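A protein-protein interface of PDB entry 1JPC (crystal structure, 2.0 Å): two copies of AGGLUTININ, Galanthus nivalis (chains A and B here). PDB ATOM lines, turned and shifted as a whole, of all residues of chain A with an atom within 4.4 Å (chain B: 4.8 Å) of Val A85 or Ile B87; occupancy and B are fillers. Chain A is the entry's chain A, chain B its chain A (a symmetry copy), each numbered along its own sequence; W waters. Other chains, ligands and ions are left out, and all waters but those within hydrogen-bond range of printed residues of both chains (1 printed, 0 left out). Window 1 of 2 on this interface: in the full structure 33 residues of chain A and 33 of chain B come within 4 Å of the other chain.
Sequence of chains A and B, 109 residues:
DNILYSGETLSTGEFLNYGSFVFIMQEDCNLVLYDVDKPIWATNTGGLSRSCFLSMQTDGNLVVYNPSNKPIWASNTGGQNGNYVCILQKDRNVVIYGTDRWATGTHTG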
ATOM      1  N   ILE A   3      24.099 -28.217  19.198  1.00  0.00           N
ATOM      2  CA  ILE A   3      24.604 -27.415  20.300  1.00  0.00           C
ATOM      3  C   ILE A   3      23.544 -27.227  21.382  1.00  0.00           C
ATOM      4  O   ILE A   3      22.367 -27.019  21.084  1.00  0.00           O
ATOM      5  CB  ILE A   3      25.028 -26.003  19.811  1.00  0.00           C
ATOM      6  CG1 ILE A   3      26.077 -26.110  18.697  1.00  0.00           C
ATOM      7  CG2 ILE A   3      25.561 -25.180  20.971  1.00  0.00           C
ATOM      8  CD1 ILE A   3      26.483 -24.792  18.104  1.00  0.00           C
ATOM      9  N   LEU A   4      23.962 -27.382  22.635  1.00  0.00           N
ATOM     10  CA  LEU A   4      23.091 -27.166  23.783  1.00  0.00           C
ATOM     11  C   LEU A   4      23.771 -25.993  24.509  1.00  0.00           C
ATOM     12  O   LEU A   4      24.913 -26.104  24.965  1.00  0.00           O
ATOM     13  CB  LEU A   4      23.033 -28.407  24.687  1.00  0.00           C
ATOM     14  CG  LEU A   4      22.114 -28.257  25.914  1.00  0.00           C
ATOM     15  CD1 LEU A   4      20.674 -28.105  25.460  1.00  0.00           C
ATOM     16  CD2 LEU A   4      22.231 -29.447  26.853  1.00  0.00           C
ATOM     17  N   TYR A   5      23.114 -24.842  24.533  1.00  0.00           N
ATOM     18  CA  TYR A   5      23.680 -23.664  25.181  1.00  0.00           C
ATOM     19  C   TYR A   5      23.405 -23.641  26.689  1.00  0.00           C
ATOM     20  O   TYR A   5      22.405 -24.195  27.154  1.00  0.00           O
ATOM     21  CB  TYR A   5      23.100 -22.405  24.555  1.00  0.00           C
ATOM     22  CG  TYR A   5      23.383 -22.260  23.083  1.00  0.00           C
ATOM     23  CD1 TYR A   5      22.584 -22.895  22.132  1.00  0.00           C
ATOM     24  CD2 TYR A   5      24.433 -21.460  22.638  1.00  0.00           C
ATOM     25  CE1 TYR A   5      22.821 -22.731  20.772  1.00  0.00           C
ATOM     26  CE2 TYR A   5      24.677 -21.286  21.286  1.00  0.00           C
ATOM     27  CZ  TYR A   5      23.872 -21.923  20.356  1.00  0.00           C
ATOM     28  OH  TYR A   5      24.117 -21.742  19.017  1.00  0.00           O
ATOM     29  N   TYR A  84      28.424 -21.035  28.362  1.00  0.00           N
ATOM     30  CA  TYR A  84      29.032 -22.294  27.932  1.00  0.00           C
ATOM     31  C   TYR A  84      28.171 -22.953  26.865  1.00  0.00           C
ATOM     32  O   TYR A  84      26.985 -22.619  26.716  1.00  0.00           O
ATOM     33  CB  TYR A  84      29.125 -23.274  29.105  1.00  0.00           C
ATOM     34  CG  TYR A  84      29.998 -22.807  30.236  1.00  0.00           C
ATOM     35  CD1 TYR A  84      29.486 -22.009  31.263  1.00  0.00           C
ATOM     36  CD2 TYR A  84      31.340 -23.169  30.289  1.00  0.00           C
ATOM     37  CE1 TYR A  84      30.296 -21.585  32.310  1.00  0.00           C
ATOM     38  CE2 TYR A  84      32.155 -22.755  31.327  1.00  0.00           C
ATOM     39  CZ  TYR A  84      31.630 -21.966  32.330  1.00  0.00           C
ATOM     40  OH  TYR A  84      32.456 -21.551  33.338  1.00  0.00           O
ATOM     41  N   VAL A  85      28.776 -23.896  26.138  1.00  0.00           N
ATOM     42  CA  VAL A  85      28.085 -24.665  25.107  1.00  0.00           C
ATOM     43  C   VAL A  85      28.555 -26.111  25.180  1.00  0.00           C
ATOM     44  O   VAL A  85      29.704 -26.382  25.550  1.00  0.00           O
ATOM     45  CB  VAL A  85      28.354 -24.156  23.651  1.00  0.00           C
ATOM     46  CG1 VAL A  85      27.718 -22.797  23.414  1.00  0.00           C
ATOM     47  CG2 VAL A  85      29.839 -24.120  23.357  1.00  0.00           C
ATOM     48  N   CYS A  86      27.626 -27.030  24.951  1.00  0.00           N
ATOM     49  CA  CYS A  86      27.931 -28.449  24.908  1.00  0.00           C
ATOM     50  C   CYS A  86      27.692 -28.786  23.436  1.00  0.00           C
ATOM     51  O   CYS A  86      26.577 -28.634  22.939  1.00  0.00           O
ATOM     52  CB  CYS A  86      26.981 -29.232  25.799  1.00  0.00           C
ATOM     53  SG  CYS A  86      27.284 -30.997  25.716  1.00  0.00           S
ATOM     54  N   ILE A  87      28.735 -29.208  22.731  1.00  0.00           N
ATOM     55  CA  ILE A  87      28.624 -29.499  21.312  1.00  0.00           C
ATOM     56  C   ILE A  87      28.840 -30.956  20.942  1.00  0.00           C
ATOM     57  O   ILE A  87      29.754 -31.603  21.462  1.00  0.00           O
ATOM     58  CB  ILE A  87      29.675 -28.674  20.504  1.00  0.00           C
ATOM     59  CG1 ILE A  87      29.598 -27.198  20.868  1.00  0.00           C
ATOM     60  CG2 ILE A  87      29.457 -28.839  18.989  1.00  0.00           C
ATOM     61  CD1 ILE A  87      30.653 -26.371  20.188  1.00  0.00           C
ATOM     62  N   VAL A  95      31.704 -32.255  23.483  1.00  0.00           N
ATOM     63  CA  VAL A  95      32.579 -31.407  24.275  1.00  0.00           C
ATOM     64  C   VAL A  95      31.887 -30.165  24.860  1.00  0.00           C
ATOM     65  O   VAL A  95      30.986 -29.607  24.239  1.00  0.00           O
ATOM     66  CB  VAL A  95      33.751 -30.929  23.377  1.00  0.00           C
ATOM     67  CG1 VAL A  95      34.825 -30.225  24.185  1.00  0.00           C
ATOM     68  CG2 VAL A  95      34.321 -32.095  22.593  1.00  0.00           C
ATOM     69  N   ILE A  96      32.307 -29.753  26.059  1.00  0.00           N
ATOM     70  CA  ILE A  96      31.787 -28.539  26.701  1.00  0.00           C
ATOM     71  C   ILE A  96      32.905 -27.483  26.578  1.00  0.00           C
ATOM     72  O   ILE A  96      34.053 -27.756  26.932  1.00  0.00           O
ATOM     73  CB  ILE A  96      31.491 -28.741  28.216  1.00  0.00           C
ATOM     74  CG1 ILE A  96      30.295 -29.662  28.425  1.00  0.00           C
ATOM     75  CG2 ILE A  96      31.220 -27.403  28.894  1.00  0.00           C
ATOM     76  CD1 ILE A  96      30.016 -29.970  29.888  1.00  0.00           C
ATOM     77  N   TYR A  97      32.596 -26.326  26.003  1.00  0.00           N
ATOM     78  CA  TYR A  97      33.573 -25.249  25.865  1.00  0.00           C
ATOM     79  C   TYR A  97      33.022 -24.043  26.603  1.00  0.00           C
ATOM     80  O   TYR A  97      31.800 -23.851  26.669  1.00  0.00           O
ATOM     81  CB  TYR A  97      33.789 -24.829  24.403  1.00  0.00           C
ATOM     82  CG  TYR A  97      34.455 -25.837  23.499  1.00  0.00           C
ATOM     83  CD1 TYR A  97      33.699 -26.770  22.791  1.00  0.00           C
ATOM     84  CD2 TYR A  97      35.830 -25.810  23.292  1.00  0.00           C
ATOM     85  CE1 TYR A  97      34.298 -27.647  21.898  1.00  0.00           C
ATOM     86  CE2 TYR A  97      36.444 -26.686  22.403  1.00  0.00           C
ATOM     87  CZ  TYR A  97      35.671 -27.599  21.709  1.00  0.00           C
ATOM     88  OH  TYR A  97      36.274 -28.463  20.829  1.00  0.00           O
ATOM     89  N   ASN B   2      27.973 -24.388  11.056  1.00  0.00           N
ATOM     90  CA  ASN B   2      27.874 -23.191  11.896  1.00  0.00           C
ATOM     91  C   ASN B   2      28.996 -23.068  12.929  1.00  0.00           C
ATOM     92  O   ASN B   2      28.982 -22.165  13.772  1.00  0.00           O
ATOM     93  CB  ASN B   2      26.508 -23.143  12.599  1.00  0.00           C
ATOM     94  CG  ASN B   2      26.313 -24.264  13.635  1.00  0.00           C
ATOM     95  OD1 ASN B   2      25.589 -24.076  14.606  1.00  0.00           O
ATOM     96  ND2 ASN B   2      26.917 -25.431  13.418  1.00  0.00           N
ATOM     97  N   ILE B   3      29.981 -23.957  12.842  1.00  0.00           N
ATOM     98  CA  ILE B   3      31.098 -23.966  13.772  1.00  0.00           C
ATOM     99  C   ILE B   3      32.434 -24.019  13.037  1.00  0.00           C
ATOM    100  O   ILE B   3      32.580 -24.731  12.043  1.00  0.00           O
ATOM    101  CB  ILE B   3      31.031 -25.203  14.710  1.00  0.00           C
ATOM    102  CG1 ILE B   3      29.698 -25.235  15.467  1.00  0.00           C
ATOM    103  CG2 ILE B   3      32.199 -25.193  15.681  1.00  0.00           C
ATOM    104  CD1 ILE B   3      29.511 -26.446  16.335  1.00  0.00           C
ATOM    105  N   VAL B  85      36.327 -22.882  19.718  1.00  0.00           N
ATOM    106  CA  VAL B  85      35.338 -22.935  18.645  1.00  0.00           C
ATOM    107  C   VAL B  85      34.765 -21.541  18.441  1.00  0.00           C
ATOM    108  O   VAL B  85      34.668 -20.754  19.391  1.00  0.00           O
ATOM    109  CB  VAL B  85      34.139 -23.900  18.936  1.00  0.00           C
ATOM    110  CG1 VAL B  85      34.585 -25.352  18.934  1.00  0.00           C
ATOM    111  CG2 VAL B  85      33.461 -23.541  20.240  1.00  0.00           C
ATOM    112  N   CYS B  86      34.508 -21.201  17.185  1.00  0.00           N
ATOM    113  CA  CYS B  86      33.887 -19.937  16.832  1.00  0.00           C
ATOM    114  C   CYS B  86      32.526 -20.384  16.298  1.00  0.00           C
ATOM    115  O   CYS B  86      32.458 -21.115  15.312  1.00  0.00           O
ATOM    116  CB  CYS B  86      34.683 -19.230  15.748  1.00  0.00           C
ATOM    117  SG  CYS B  86      33.907 -17.697  15.238  1.00  0.00           S
ATOM    118  N   ILE B  87      31.450 -19.978  16.961  1.00  0.00           N
ATOM    119  CA  ILE B  87      30.115 -20.395  16.568  1.00  0.00           C
ATOM    120  C   ILE B  87      29.214 -19.273  16.081  1.00  0.00           C
ATOM    121  O   ILE B  87      29.189 -18.190  16.674  1.00  0.00           O
ATOM    122  CB  ILE B  87      29.378 -21.067  17.770  1.00  0.00           C
ATOM    123  CG1 ILE B  87      30.239 -22.158  18.388  1.00  0.00           C
ATOM    124  CG2 ILE B  87      28.032 -21.667  17.324  1.00  0.00           C
ATOM    125  CD1 ILE B  87      29.616 -22.774  19.610  1.00  0.00           C
ATOM    126  N   LEU B  88      28.519 -19.521  14.971  1.00  0.00           N
ATOM    127  CA  LEU B  88      27.525 -18.583  14.445  1.00  0.00           C
ATOM    128  C   LEU B  88      26.272 -19.177  15.094  1.00  0.00           C
ATOM    129  O   LEU B  88      25.749 -20.207  14.649  1.00  0.00           O
ATOM    130  CB  LEU B  88      27.418 -18.648  12.915  1.00  0.00           C
ATOM    131  CG  LEU B  88      26.143 -18.091  12.245  1.00  0.00           C
ATOM    132  CD1 LEU B  88      25.715 -16.769  12.840  1.00  0.00           C
ATOM    133  CD2 LEU B  88      26.372 -17.936  10.751  1.00  0.00           C
ATOM    134  N   GLN B  89      25.839 -18.555  16.185  1.00  0.00           N
ATOM    135  CA  GLN B  89      24.709 -19.045  16.966  1.00  0.00           C
ATOM    136  C   GLN B  89      23.329 -18.772  16.402  1.00  0.00           C
ATOM    137  O   GLN B  89      23.127 -17.870  15.590  1.00  0.00           O
ATOM    138  CB  GLN B  89      24.777 -18.500  18.405  1.00  0.00           C
ATOM    139  CG  GLN B  89      26.159 -18.542  19.035  1.00  0.00           C
ATOM    140  CD  GLN B  89      26.177 -18.164  20.508  1.00  0.00           C
ATOM    141  OE1 GLN B  89      27.034 -18.628  21.248  1.00  0.00           O
ATOM    142  NE2 GLN B  89      25.241 -17.321  20.937  1.00  0.00           N
ATOM    143  N   ASN B  93      24.418 -14.272  17.123  1.00  0.00           N
ATOM    144  CA  ASN B  93      25.680 -13.785  17.683  1.00  0.00           C
ATOM    145  C   ASN B  93      26.766 -14.738  17.178  1.00  0.00           C
ATOM    146  O   ASN B  93      26.495 -15.914  16.928  1.00  0.00           O
ATOM    147  CB  ASN B  93      25.635 -13.820  19.225  1.00  0.00           C
ATOM    148  CG  ASN B  93      26.502 -12.747  19.873  1.00  0.00           C
ATOM    149  OD1 ASN B  93      27.197 -12.001  19.199  1.00  0.00           O
ATOM    150  ND2 ASN B  93      26.436 -12.651  21.187  1.00  0.00           N
ATOM    151  N   VAL B  94      27.956 -14.208  16.918  1.00  0.00           N
ATOM    152  CA  VAL B  94      29.089 -15.019  16.494  1.00  0.00           C
ATOM    153  C   VAL B  94      29.967 -14.944  17.739  1.00  0.00           C
ATOM    154  O   VAL B  94      30.395 -13.860  18.139  1.00  0.00           O
ATOM    155  CB  VAL B  94      29.807 -14.410  15.281  1.00  0.00           C
ATOM    156  CG1 VAL B  94      31.028 -15.229  14.948  1.00  0.00           C
ATOM    157  CG2 VAL B  94      28.858 -14.347  14.098  1.00  0.00           C
ATOM    158  N   VAL B  95      30.202 -16.088  18.367  1.00  0.00           N
ATOM    159  CA  VAL B  95      30.951 -16.141  19.611  1.00  0.00           C
ATOM    160  C   VAL B  95      32.105 -17.157  19.605  1.00  0.00           C
ATOM    161  O   VAL B  95      32.006 -18.205  18.972  1.00  0.00           O
ATOM    162  CB  VAL B  95      29.979 -16.521  20.759  1.00  0.00           C
ATOM    163  CG1 VAL B  95      30.635 -16.378  22.120  1.00  0.00           C
ATOM    164  CG2 VAL B  95      28.709 -15.698  20.666  1.00  0.00           C
ATOM    165  N   TYR B  97      34.257 -19.595  22.049  1.00  0.00           N
ATOM    166  CA  TYR B  97      34.227 -20.208  23.374  1.00  0.00           C
ATOM    167  C   TYR B  97      35.466 -21.079  23.496  1.00  0.00           C
ATOM    168  O   TYR B  97      35.944 -21.634  22.498  1.00  0.00           O
ATOM    169  CB  TYR B  97      33.008 -21.120  23.578  1.00  0.00           C
ATOM    170  CG  TYR B  97      31.659 -20.447  23.625  1.00  0.00           C
ATOM    171  CD1 TYR B  97      30.920 -20.246  22.460  1.00  0.00           C
ATOM    172  CD2 TYR B  97      31.086 -20.080  24.839  1.00  0.00           C
ATOM    173  CE1 TYR B  97      29.646 -19.699  22.505  1.00  0.00           C
ATOM    174  CE2 TYR B  97      29.812 -19.528  24.899  1.00  0.00           C
ATOM    175  CZ  TYR B  97      29.097 -19.343  23.729  1.00  0.00           C
ATOM    176  OH  TYR B  97      27.837 -18.800  23.785  1.00  0.00           O
HETATM  177  O   HOH W   1      26.365 -20.147  25.657  1.00  0.00           O
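Among the printed residues, pairs that only touch across the chains: Tyr A5 with Gln B89 (3.4 Å), Ile A87 with Ile B3 (3.6 Å), Ile A3 with Ile B87 (3.6 Å), Ile A3 with Asn B2 (3.7 Å), Tyr A97 with Val B85 (3.7 Å), Val A85 with Tyr B97 (3.7 Å), Ile A87 with Ile B87 (3.8 Å), Ile A3 with Ile B3 (3.9 Å), Tyr A97 with Tyr B97 (3.9 Å), Ile A87 with Val B85 (3.99 Å) and Val A85 with Ile B87 (3.99 Å).
Ile A3 touches its own counterpart, Ile B3. Val A85 touches Ile B87, and with the chains exchanged Ile A87 touches Val B85. Val A85 touches Tyr B97, and with the chains exchanged Tyr A97 touches Val B85. Ile A87 touches its own counterpart, Ile B87. Positions printed for both chains: 3, 85, 86, 87, 95 and 97. Of the 11 pairs that touch across the chains among the printed residues, 9 have their exchanged pair printed and touching as well.
Of the 10 printed residues of chain A, 5 touch a printed residue of chain B. Hydrophobic or aromatic side chains of chain B that line the printed part of chain A: Ile B3, Val B85, Ile B87 and Tyr B97. Among the printed residues, no Asp or Glu carboxylate lies within 4 Å of a Lys or Arg side-chain nitrogen of the other chain.
The backbone carbonyl oxygen (O) of Val A85 lies within hydrogen-bond range of the backbone NH (N) of Tyr A97, at 2.9 Å. N of Ile A87 is in hydrogen-bond range of O of Val A95. The backbone NH (N) of Leu B88 sits at hydrogen-bond distance from the backbone carbonyl oxygen (O) of Asn B2. O of Val B85 sits at hydrogen-bond distance from N of Tyr B97 (2.9 Å). N of Ile B87 lies within hydrogen-bond range of O of Val B95 (2.7 Å). OE1 of Gln B89 is in hydrogen-bond range of OH of Tyr B97.
Water W1 bridges OH of Tyr B97 (2.7 Å) and O of Tyr A84 (2.8 Å).
Of the printed residues of chain B, Val A85 touches Ile B87 and Tyr B97. Printed residues of chain A within 4 Å of Ile B87: Ile A3 (3.6 Å), Val A85 (3.99 Å) and Ile A87 (3.8 Å). Printed residues of chain A within 4 Å of Asn B2: Ile A3 (3.7 Å). Printed residues of chain A within 4 Å of Ile B3: Ile A3 (3.9 Å) and Ile A87 (3.6 Å). Val B95 touches none of the printed residues of chain A. The nearest printed residue of chain B that does not touch Val A85 is Gln B89 (4.7 Å).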
